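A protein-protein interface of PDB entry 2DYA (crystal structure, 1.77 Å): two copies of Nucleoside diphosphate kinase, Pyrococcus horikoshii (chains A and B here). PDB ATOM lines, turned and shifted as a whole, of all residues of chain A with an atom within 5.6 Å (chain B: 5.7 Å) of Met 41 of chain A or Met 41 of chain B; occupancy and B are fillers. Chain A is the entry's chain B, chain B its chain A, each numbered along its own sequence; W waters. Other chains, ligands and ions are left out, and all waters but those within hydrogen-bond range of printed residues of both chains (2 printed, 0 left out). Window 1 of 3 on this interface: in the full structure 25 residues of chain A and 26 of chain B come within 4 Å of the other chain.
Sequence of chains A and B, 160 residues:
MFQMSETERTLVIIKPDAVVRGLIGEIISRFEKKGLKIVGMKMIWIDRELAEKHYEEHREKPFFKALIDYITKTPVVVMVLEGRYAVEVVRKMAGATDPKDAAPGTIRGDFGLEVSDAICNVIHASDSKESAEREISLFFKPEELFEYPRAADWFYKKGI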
ATOM      1  N   ILE A  24      -5.005  22.998  -4.344  1.00  0.00           N
ATOM      2  CA  ILE A  24      -5.342  22.491  -3.015  1.00  0.00           C
ATOM      3  C   ILE A  24      -6.793  22.738  -2.619  1.00  0.00           C
ATOM      4  O   ILE A  24      -7.498  21.810  -2.208  1.00  0.00           O
ATOM      5  CB  ILE A  24      -4.445  23.118  -1.925  1.00  0.00           C
ATOM      6  CG1 ILE A  24      -2.984  22.714  -2.148  1.00  0.00           C
ATOM      7  CG2 ILE A  24      -4.920  22.667  -0.548  1.00  0.00           C
ATOM      8  CD1 ILE A  24      -2.010  23.432  -1.233  1.00  0.00           C
ATOM      9  N   ILE A  28      -9.966  20.023  -1.974  1.00  0.00           N
ATOM     10  CA  ILE A  28     -10.610  19.945  -0.662  1.00  0.00           C
ATOM     11  C   ILE A  28     -12.124  20.195  -0.769  1.00  0.00           C
ATOM     12  O   ILE A  28     -12.919  19.492  -0.148  1.00  0.00           O
ATOM     13  CB  ILE A  28      -9.998  20.971   0.334  1.00  0.00           C
ATOM     14  CG1 ILE A  28      -8.558  20.574   0.671  1.00  0.00           C
ATOM     15  CG2 ILE A  28     -10.836  21.034   1.609  1.00  0.00           C
ATOM     16  CD1 ILE A  28      -7.779  21.638   1.422  1.00  0.00           C
ATOM     17  N   ILE A  38     -13.229  16.357   7.216  1.00  0.00           N
ATOM     18  CA  ILE A  38     -11.778  16.448   7.343  1.00  0.00           C
ATOM     19  C   ILE A  38     -11.441  16.368   8.837  1.00  0.00           C
ATOM     20  O   ILE A  38     -11.637  17.337   9.573  1.00  0.00           O
ATOM     21  CB  ILE A  38     -11.248  17.790   6.783  1.00  0.00           C
ATOM     22  CG1 ILE A  38     -11.641  17.932   5.313  1.00  0.00           C
ATOM     23  CG2 ILE A  38      -9.738  17.858   6.932  1.00  0.00           C
ATOM     24  CD1 ILE A  38     -11.321  19.289   4.718  1.00  0.00           C
ATOM     25  N   VAL A  39     -10.946  15.217   9.285  1.00  0.00           N
ATOM     26  CA  VAL A  39     -10.609  15.049  10.697  1.00  0.00           C
ATOM     27  C   VAL A  39      -9.133  15.325  10.991  1.00  0.00           C
ATOM     28  O   VAL A  39      -8.734  15.474  12.150  1.00  0.00           O
ATOM     29  CB  VAL A  39     -10.984  13.630  11.196  1.00  0.00           C
ATOM     30  CG1 VAL A  39     -12.493  13.425  11.071  1.00  0.00           C
ATOM     31  CG2 VAL A  39     -10.223  12.574  10.414  1.00  0.00           C
ATOM     32  N   GLY A  40      -8.331  15.404   9.933  1.00  0.00           N
ATOM     33  CA  GLY A  40      -6.913  15.679  10.078  1.00  0.00           C
ATOM     34  C   GLY A  40      -6.380  16.280   8.791  1.00  0.00           C
ATOM     35  O   GLY A  40      -6.856  15.933   7.708  1.00  0.00           O
ATOM     36  N   MET A  41      -5.401  17.180   8.898  1.00  0.00           N
ATOM     37  CA  MET A  41      -4.819  17.816   7.719  1.00  0.00           C
ATOM     38  C   MET A  41      -3.625  18.702   8.051  1.00  0.00           C
ATOM     39  O   MET A  41      -3.607  19.385   9.078  1.00  0.00           O
ATOM     40  CB  MET A  41      -5.877  18.651   6.989  1.00  0.00           C
ATOM     41  CG  MET A  41      -5.327  19.454   5.818  1.00  0.00           C
ATOM     42  SD  MET A  41      -6.595  20.366   4.922  1.00  0.00           S
ATOM     43  CE  MET A  41      -6.625  21.875   5.853  1.00  0.00           C
ATOM     44  N   LYS A  42      -2.631  18.694   7.168  1.00  0.00           N
ATOM     45  CA  LYS A  42      -1.437  19.504   7.361  1.00  0.00           C
ATOM     46  C   LYS A  42      -0.512  19.488   6.147  1.00  0.00           C
ATOM     47  O   LYS A  42      -0.466  18.514   5.389  1.00  0.00           O
ATOM     48  CB  LYS A  42      -0.660  19.008   8.581  1.00  0.00           C
ATOM     49  CG  LYS A  42      -0.204  17.567   8.463  1.00  0.00           C
ATOM     50  CD  LYS A  42       0.556  17.129   9.702  1.00  0.00           C
ATOM     51  CE  LYS A  42       1.045  15.700   9.561  1.00  0.00           C
ATOM     52  NZ  LYS A  42       1.745  15.217  10.789  1.00  0.00           N
ATOM     53  N   MET A  43       0.219  20.580   5.963  1.00  0.00           N
ATOM     54  CA  MET A  43       1.168  20.658   4.873  1.00  0.00           C
ATOM     55  C   MET A  43       2.514  20.220   5.434  1.00  0.00           C
ATOM     56  O   MET A  43       2.969  20.729   6.467  1.00  0.00           O
ATOM     57  CB  MET A  43       1.279  22.081   4.330  1.00  0.00           C
ATOM     58  CG  MET A  43       2.395  22.233   3.302  1.00  0.00           C
ATOM     59  SD  MET A  43       2.495  23.858   2.558  1.00  0.00           S
ATOM     60  CE  MET A  43       1.239  23.695   1.290  1.00  0.00           C
ATOM     61  N   VAL A  77       0.033  18.200   0.899  1.00  0.00           N
ATOM     62  CA  VAL A  77      -0.957  18.397   1.939  1.00  0.00           C
ATOM     63  C   VAL A  77      -1.553  17.021   2.178  1.00  0.00           C
ATOM     64  O   VAL A  77      -2.162  16.439   1.281  1.00  0.00           O
ATOM     65  CB  VAL A  77      -2.070  19.384   1.510  1.00  0.00           C
ATOM     66  CG1 VAL A  77      -3.142  19.469   2.602  1.00  0.00           C
ATOM     67  CG2 VAL A  77      -1.472  20.760   1.260  1.00  0.00           C
ATOM     68  N   VAL A  78      -1.326  16.483   3.372  1.00  0.00           N
ATOM     69  CA  VAL A  78      -1.869  15.180   3.729  1.00  0.00           C
ATOM     70  C   VAL A  78      -3.110  15.457   4.557  1.00  0.00           C
ATOM     71  O   VAL A  78      -3.163  16.427   5.310  1.00  0.00           O
ATOM     72  CB  VAL A  78      -0.860  14.333   4.557  1.00  0.00           C
ATOM     73  CG1 VAL A  78       0.326  13.946   3.691  1.00  0.00           C
ATOM     74  CG2 VAL A  78      -0.393  15.112   5.794  1.00  0.00           C
ATOM     75  N   MET A  79      -4.126  14.624   4.395  1.00  0.00           N
ATOM     76  CA  MET A  79      -5.353  14.820   5.146  1.00  0.00           C
ATOM     77  C   MET A  79      -6.091  13.511   5.307  1.00  0.00           C
ATOM     78  O   MET A  79      -5.938  12.589   4.501  1.00  0.00           O
ATOM     79  CB  MET A  79      -6.251  15.851   4.451  1.00  0.00           C
ATOM     80  CG  MET A  79      -6.880  15.393   3.153  1.00  0.00           C
ATOM     81  SD  MET A  79      -7.570  16.784   2.203  1.00  0.00           S
ATOM     82  CE  MET A  79      -8.858  17.363   3.301  1.00  0.00           C
ATOM     83  N   VAL A  80      -6.876  13.431   6.371  1.00  0.00           N
ATOM     84  CA  VAL A  80      -7.648  12.240   6.651  1.00  0.00           C
ATOM     85  C   VAL A  80      -9.118  12.579   6.495  1.00  0.00           C
ATOM     86  O   VAL A  80      -9.632  13.502   7.136  1.00  0.00           O
ATOM     87  CB  VAL A  80      -7.385  11.725   8.074  1.00  0.00           C
ATOM     88  CG1 VAL A  80      -8.282  10.529   8.360  1.00  0.00           C
ATOM     89  CG2 VAL A  80      -5.918  11.340   8.216  1.00  0.00           C
ATOM     90  N   PHE A 140      -0.063  10.745  10.468  1.00  0.00           N
ATOM     91  CA  PHE A 140      -0.753  11.399  11.576  1.00  0.00           C
ATOM     92  C   PHE A 140      -0.693  10.718  12.936  1.00  0.00           C
ATOM     93  O   PHE A 140      -0.805   9.499  13.045  1.00  0.00           O
ATOM     94  CB  PHE A 140      -2.234  11.610  11.209  1.00  0.00           C
ATOM     95  CG  PHE A 140      -2.461  12.618  10.110  1.00  0.00           C
ATOM     96  CD1 PHE A 140      -2.618  13.971  10.408  1.00  0.00           C
ATOM     97  CD2 PHE A 140      -2.506  12.218   8.778  1.00  0.00           C
ATOM     98  CE1 PHE A 140      -2.820  14.914   9.395  1.00  0.00           C
ATOM     99  CE2 PHE A 140      -2.706  13.153   7.755  1.00  0.00           C
ATOM    100  CZ  PHE A 140      -2.864  14.503   8.068  1.00  0.00           C
ATOM    101  N   GLU A 144      -3.528  14.518  16.264  1.00  0.00           N
ATOM    102  CA  GLU A 144      -3.741  15.381  15.104  1.00  0.00           C
ATOM    103  C   GLU A 144      -5.052  15.064  14.391  1.00  0.00           C
ATOM    104  O   GLU A 144      -5.378  15.675  13.377  1.00  0.00           O
ATOM    105  CB  GLU A 144      -2.594  15.219  14.112  1.00  0.00           C
ATOM    106  CG  GLU A 144      -1.232  15.614  14.651  1.00  0.00           C
ATOM    107  CD  GLU A 144      -0.122  15.334  13.656  1.00  0.00           C
ATOM    108  OE1 GLU A 144       0.135  14.148  13.368  1.00  0.00           O
ATOM    109  OE2 GLU A 144       0.490  16.298  13.155  1.00  0.00           O
ATOM    110  N   ILE B  24     -13.636  25.342   3.869  1.00  0.00           N
ATOM    111  CA  ILE B  24     -12.170  25.350   3.875  1.00  0.00           C
ATOM    112  C   ILE B  24     -11.564  25.442   2.475  1.00  0.00           C
ATOM    113  O   ILE B  24     -10.719  26.300   2.212  1.00  0.00           O
ATOM    114  CB  ILE B  24     -11.605  24.077   4.560  1.00  0.00           C
ATOM    115  CG1 ILE B  24     -12.097  24.001   6.008  1.00  0.00           C
ATOM    116  CG2 ILE B  24     -10.075  24.083   4.507  1.00  0.00           C
ATOM    117  CD1 ILE B  24     -11.682  22.732   6.741  1.00  0.00           C
ATOM    118  N   ILE B  28      -9.460  28.597   0.757  1.00  0.00           N
ATOM    119  CA  ILE B  28      -8.086  28.353   0.314  1.00  0.00           C
ATOM    120  C   ILE B  28      -7.919  28.686  -1.171  1.00  0.00           C
ATOM    121  O   ILE B  28      -6.915  29.268  -1.571  1.00  0.00           O
ATOM    122  CB  ILE B  28      -7.667  26.871   0.529  1.00  0.00           C
ATOM    123  CG1 ILE B  28      -7.511  26.579   2.021  1.00  0.00           C
ATOM    124  CG2 ILE B  28      -6.355  26.583  -0.196  1.00  0.00           C
ATOM    125  CD1 ILE B  28      -7.164  25.137   2.321  1.00  0.00           C
ATOM    126  N   ILE B  38       0.860  29.062  -0.122  1.00  0.00           N
ATOM    127  CA  ILE B  38       0.654  28.430   1.173  1.00  0.00           C
ATOM    128  C   ILE B  38       2.009  27.849   1.568  1.00  0.00           C
ATOM    129  O   ILE B  38       2.487  26.901   0.951  1.00  0.00           O
ATOM    130  CB  ILE B  38      -0.387  27.284   1.086  1.00  0.00           C
ATOM    131  CG1 ILE B  38      -1.723  27.834   0.585  1.00  0.00           C
ATOM    132  CG2 ILE B  38      -0.567  26.626   2.458  1.00  0.00           C
ATOM    133  CD1 ILE B  38      -2.782  26.766   0.375  1.00  0.00           C
ATOM    134  N   VAL B  39       2.639  28.433   2.583  1.00  0.00           N
ATOM    135  CA  VAL B  39       3.942  27.952   3.030  1.00  0.00           C
ATOM    136  C   VAL B  39       3.843  27.176   4.336  1.00  0.00           C
ATOM    137  O   VAL B  39       4.843  26.675   4.847  1.00  0.00           O
ATOM    138  CB  VAL B  39       4.942  29.117   3.197  1.00  0.00           C
ATOM    139  CG1 VAL B  39       5.159  29.803   1.851  1.00  0.00           C
ATOM    140  CG2 VAL B  39       4.427  30.108   4.234  1.00  0.00           C
ATOM    141  N   GLY B  40       2.626  27.071   4.862  1.00  0.00           N
ATOM    142  CA  GLY B  40       2.397  26.345   6.101  1.00  0.00           C
ATOM    143  C   GLY B  40       0.907  26.195   6.342  1.00  0.00           C
ATOM    144  O   GLY B  40       0.138  27.107   6.029  1.00  0.00           O
ATOM    145  N   MET B  41       0.490  25.057   6.893  1.00  0.00           N
ATOM    146  CA  MET B  41      -0.933  24.824   7.142  1.00  0.00           C
ATOM    147  C   MET B  41      -1.205  23.541   7.915  1.00  0.00           C
ATOM    148  O   MET B  41      -0.504  22.539   7.744  1.00  0.00           O
ATOM    149  CB  MET B  41      -1.689  24.780   5.807  1.00  0.00           C
ATOM    150  CG  MET B  41      -3.161  24.408   5.911  1.00  0.00           C
ATOM    151  SD  MET B  41      -3.990  24.530   4.308  1.00  0.00           S
ATOM    152  CE  MET B  41      -3.546  22.968   3.566  1.00  0.00           C
ATOM    153  N   LYS B  42      -2.233  23.574   8.762  1.00  0.00           N
ATOM    154  CA  LYS B  42      -2.599  22.402   9.553  1.00  0.00           C
ATOM    155  C   LYS B  42      -3.899  22.585  10.319  1.00  0.00           C
ATOM    156  O   LYS B  42      -4.226  23.686  10.768  1.00  0.00           O
ATOM    157  CB  LYS B  42      -1.483  22.068  10.551  1.00  0.00           C
ATOM    158  CG  LYS B  42      -1.243  23.163  11.579  1.00  0.00           C
ATOM    159  CD  LYS B  42      -0.040  22.854  12.449  1.00  0.00           C
ATOM    160  CE  LYS B  42       0.148  23.911  13.523  1.00  0.00           C
ATOM    161  NZ  LYS B  42       1.262  23.555  14.443  1.00  0.00           N
ATOM    162  N   MET B  43      -4.647  21.496  10.455  1.00  0.00           N
ATOM    163  CA  MET B  43      -5.885  21.532  11.216  1.00  0.00           C
ATOM    164  C   MET B  43      -5.486  21.270  12.666  1.00  0.00           C
ATOM    165  O   MET B  43      -4.747  20.325  12.963  1.00  0.00           O
ATOM    166  CB  MET B  43      -6.862  20.453  10.740  1.00  0.00           C
ATOM    167  CG  MET B  43      -8.113  20.342  11.614  1.00  0.00           C
ATOM    168  SD  MET B  43      -9.369  19.192  10.985  1.00  0.00           S
ATOM    169  CE  MET B  43     -10.322  20.293   9.901  1.00  0.00           C
ATOM    170  N   VAL B  77      -8.335  25.646  10.802  1.00  0.00           N
ATOM    171  CA  VAL B  77      -7.203  25.421   9.916  1.00  0.00           C
ATOM    172  C   VAL B  77      -6.363  26.696   9.982  1.00  0.00           C
ATOM    173  O   VAL B  77      -6.831  27.775   9.608  1.00  0.00           O
ATOM    174  CB  VAL B  77      -7.639  25.170   8.446  1.00  0.00           C
ATOM    175  CG1 VAL B  77      -6.407  24.922   7.574  1.00  0.00           C
ATOM    176  CG2 VAL B  77      -8.572  23.984   8.370  1.00  0.00           C
ATOM    177  N   VAL B  78      -5.148  26.589  10.509  1.00  0.00           N
ATOM    178  CA  VAL B  78      -4.273  27.749  10.574  1.00  0.00           C
ATOM    179  C   VAL B  78      -3.301  27.602   9.421  1.00  0.00           C
ATOM    180  O   VAL B  78      -2.809  26.508   9.156  1.00  0.00           O
ATOM    181  CB  VAL B  78      -3.497  27.830  11.917  1.00  0.00           C
ATOM    182  CG1 VAL B  78      -4.469  28.095  13.053  1.00  0.00           C
ATOM    183  CG2 VAL B  78      -2.718  26.547  12.170  1.00  0.00           C
ATOM    184  N   MET B  79      -3.046  28.690   8.712  1.00  0.00           N
ATOM    185  CA  MET B  79      -2.133  28.626   7.583  1.00  0.00           C
ATOM    186  C   MET B  79      -1.393  29.937   7.400  1.00  0.00           C
ATOM    187  O   MET B  79      -1.864  30.999   7.813  1.00  0.00           O
ATOM    188  CB  MET B  79      -2.893  28.262   6.297  1.00  0.00           C
ATOM    189  CG  MET B  79      -3.834  29.339   5.771  1.00  0.00           C
ATOM    190  SD  MET B  79      -4.938  28.735   4.456  1.00  0.00           S
ATOM    191  CE  MET B  79      -3.800  28.543   3.114  1.00  0.00           C
ATOM    192  N   VAL B  80      -0.221  29.847   6.785  1.00  0.00           N
ATOM    193  CA  VAL B  80       0.606  31.012   6.538  1.00  0.00           C
ATOM    194  C   VAL B  80       0.645  31.228   5.034  1.00  0.00           C
ATOM    195  O   VAL B  80       0.984  30.318   4.275  1.00  0.00           O
ATOM    196  CB  VAL B  80       2.042  30.795   7.065  1.00  0.00           C
ATOM    197  CG1 VAL B  80       2.870  32.053   6.853  1.00  0.00           C
ATOM    198  CG2 VAL B  80       2.002  30.404   8.544  1.00  0.00           C
ATOM    199  N   PHE B 140       3.072  27.886  14.586  1.00  0.00           N
ATOM    200  CA  PHE B 140       4.026  27.070  13.829  1.00  0.00           C
ATOM    201  C   PHE B 140       5.482  27.109  14.294  1.00  0.00           C
ATOM    202  O   PHE B 140       5.955  28.120  14.815  1.00  0.00           O
ATOM    203  CB  PHE B 140       4.006  27.492  12.349  1.00  0.00           C
ATOM    204  CG  PHE B 140       2.688  27.264  11.655  1.00  0.00           C
ATOM    205  CD1 PHE B 140       2.433  26.065  10.992  1.00  0.00           C
ATOM    206  CD2 PHE B 140       1.706  28.253  11.653  1.00  0.00           C
ATOM    207  CE1 PHE B 140       1.220  25.855  10.334  1.00  0.00           C
ATOM    208  CE2 PHE B 140       0.485  28.055  10.999  1.00  0.00           C
ATOM    209  CZ  PHE B 140       0.244  26.855  10.338  1.00  0.00           C
ATOM    210  N   GLU B 144       7.702  23.696  10.149  1.00  0.00           N
ATOM    211  CA  GLU B 144       6.369  23.524   9.583  1.00  0.00           C
ATOM    212  C   GLU B 144       6.099  24.571   8.504  1.00  0.00           C
ATOM    213  O   GLU B 144       4.999  24.647   7.948  1.00  0.00           O
ATOM    214  CB  GLU B 144       5.321  23.625  10.693  1.00  0.00           C
ATOM    215  CG  GLU B 144       5.386  22.492  11.705  1.00  0.00           C
ATOM    216  CD  GLU B 144       4.450  22.717  12.873  1.00  0.00           C
ATOM    217  OE1 GLU B 144       4.674  23.682  13.629  1.00  0.00           O
ATOM    218  OE2 GLU B 144       3.488  21.938  13.034  1.00  0.00           O
HETATM  219  O   HOH W   1       2.804  23.297   7.688  1.00  0.00           O
HETATM  220  O   HOH W   2      -4.581  17.745  11.561  1.00  0.00           O
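O of Val 80 of chain B sits at hydrogen-bond distance from N of Val 39 of chain B, 3.0 Å away. The backbone carbonyl oxygen (O) of Gly 40 of chain B sits at hydrogen-bond distance from the backbone NH (N) of Val 80 of chain B (2.9 Å). N of Lys 42 of chain B lies within hydrogen-bond range of O of Val 78 of chain B. The side-chain amino group of Lys 42 of chain B is in salt-bridge range of the side-chain carboxylate of Glu 144 of chain B. The backbone NH of Val 39 of chain A lies within hydrogen-bond range of the backbone carbonyl oxygen of Val 80 of chain A (3.0 Å). The backbone carbonyl oxygen (O) of Val 78 of chain A is in hydrogen-bond range of the backbone NH (N) of Lys 42 of chain A, at 3.0 Å.
Ile 24 of chain A touches Ile 38 of chain B, but with the chains exchanged Ile 38 of chain A does not touch Ile 24 of chain B (4.01 Å). Ile 28 of chain B touches its own counterpart, Ile 28 of chain A. Met 41 of chain B touches its own counterpart, Met 41 of chain A. Met 41 of chain A touches Val 77 of chain B, and with the chains exchanged Val 77 of chain A touches Met 41 of chain B. 14 positions are printed for both chains.
Hydrophobic or aromatic side chains of chain B within 4 Å of the printed part of chain A: Ile 28, Ile 38, Met 41, Met 43 and Val 77. Along chain B the printed residues that touch a printed residue of chain A span positions 28 to 77. Of the 14 printed residues of chain A, 8 touch a printed residue of chain B. Printed residues of chain A that touch a printed residue of chain B: Ile 24, Ile 28, Ile 38, Val 39, Met 41, Lys 42, Met 43 and Val 77. Hydrophobic or aromatic side chains of chain A within 4 Å of the printed part of chain B: Ile 24, Ile 28, Ile 38, Met 41, Met 43 and Val 77. Along chain A the printed residues that touch a printed residue of chain B span positions 24 to 77. Among the printed residues, 15 pairs touch across the chains. Among the printed residues, no Asp or Glu carboxylate lies within 4 Å of a Lys or Arg side-chain nitrogen of the other chain.
Water W1 lies within hydrogen-bond range of the backbone carbonyl oxygen (O) of Glu 144 of chain B, the backbone carbonyl oxygen (O) of Met 43 of chain A and the backbone NH (N) of Met 41 of chain B. Water W2 lies within hydrogen-bond range of N of Met 41 of chain A (2.8 Å), O of Glu 144 of chain A (2.9 Å) and O of Met 43 of chain B (2.9 Å).
O of Met 41 of chain B is in hydrogen-bond range of N of Met 43 of chain A (2.7 Å). N of Met 43 of chain B is in hydrogen-bond range of O of Met 41 of chain A (2.7 Å). SD of Met 43 of chain B sits close to O of Ile 38 of chain A (3.3 Å). O of Ile 38 of chain B lies close to SD of Met 43 of chain A (3.4 Å).
Among the printed residues, pairs that only touch across the chains: Ile 24 of chain A with Ile 38 of chain B, Ile 28 of chain A with Ile 28 of chain B, Val 39 of chain A with Met 43 of chain B, Met 41 of chain A with Met 41 of chain B, Met 41 of chain A with Lys 42 of chain B, Met 41 of chain A with Val 77 of chain B, Lys 42 of chain A with Met 41 of chain B, Lys 42 of chain A with Lys 42 of chain B, Met 43 of chain A with Val 39 of chain B, Met 43 of chain A with Gly 40 of chain B and Val 77 of chain A with Met 41 of chain B.
Of the printed residues of chain A, Met 41 of chain B touches Met 41 (3.99 Å), Lys 42 (3.2 Å), Met 43 (2.7 Å) and Val 77 (3.7 Å). Of the printed residues of chain B, Ile 38 of chain A touches Met 43. Of the printed residues of chain A, Val 77 of chain B touches Met 41 (3.5 Å). The nearest printed residue of chain B that does not touch Met 43 of chain A is Glu 144 of chain B (4.7 Å).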
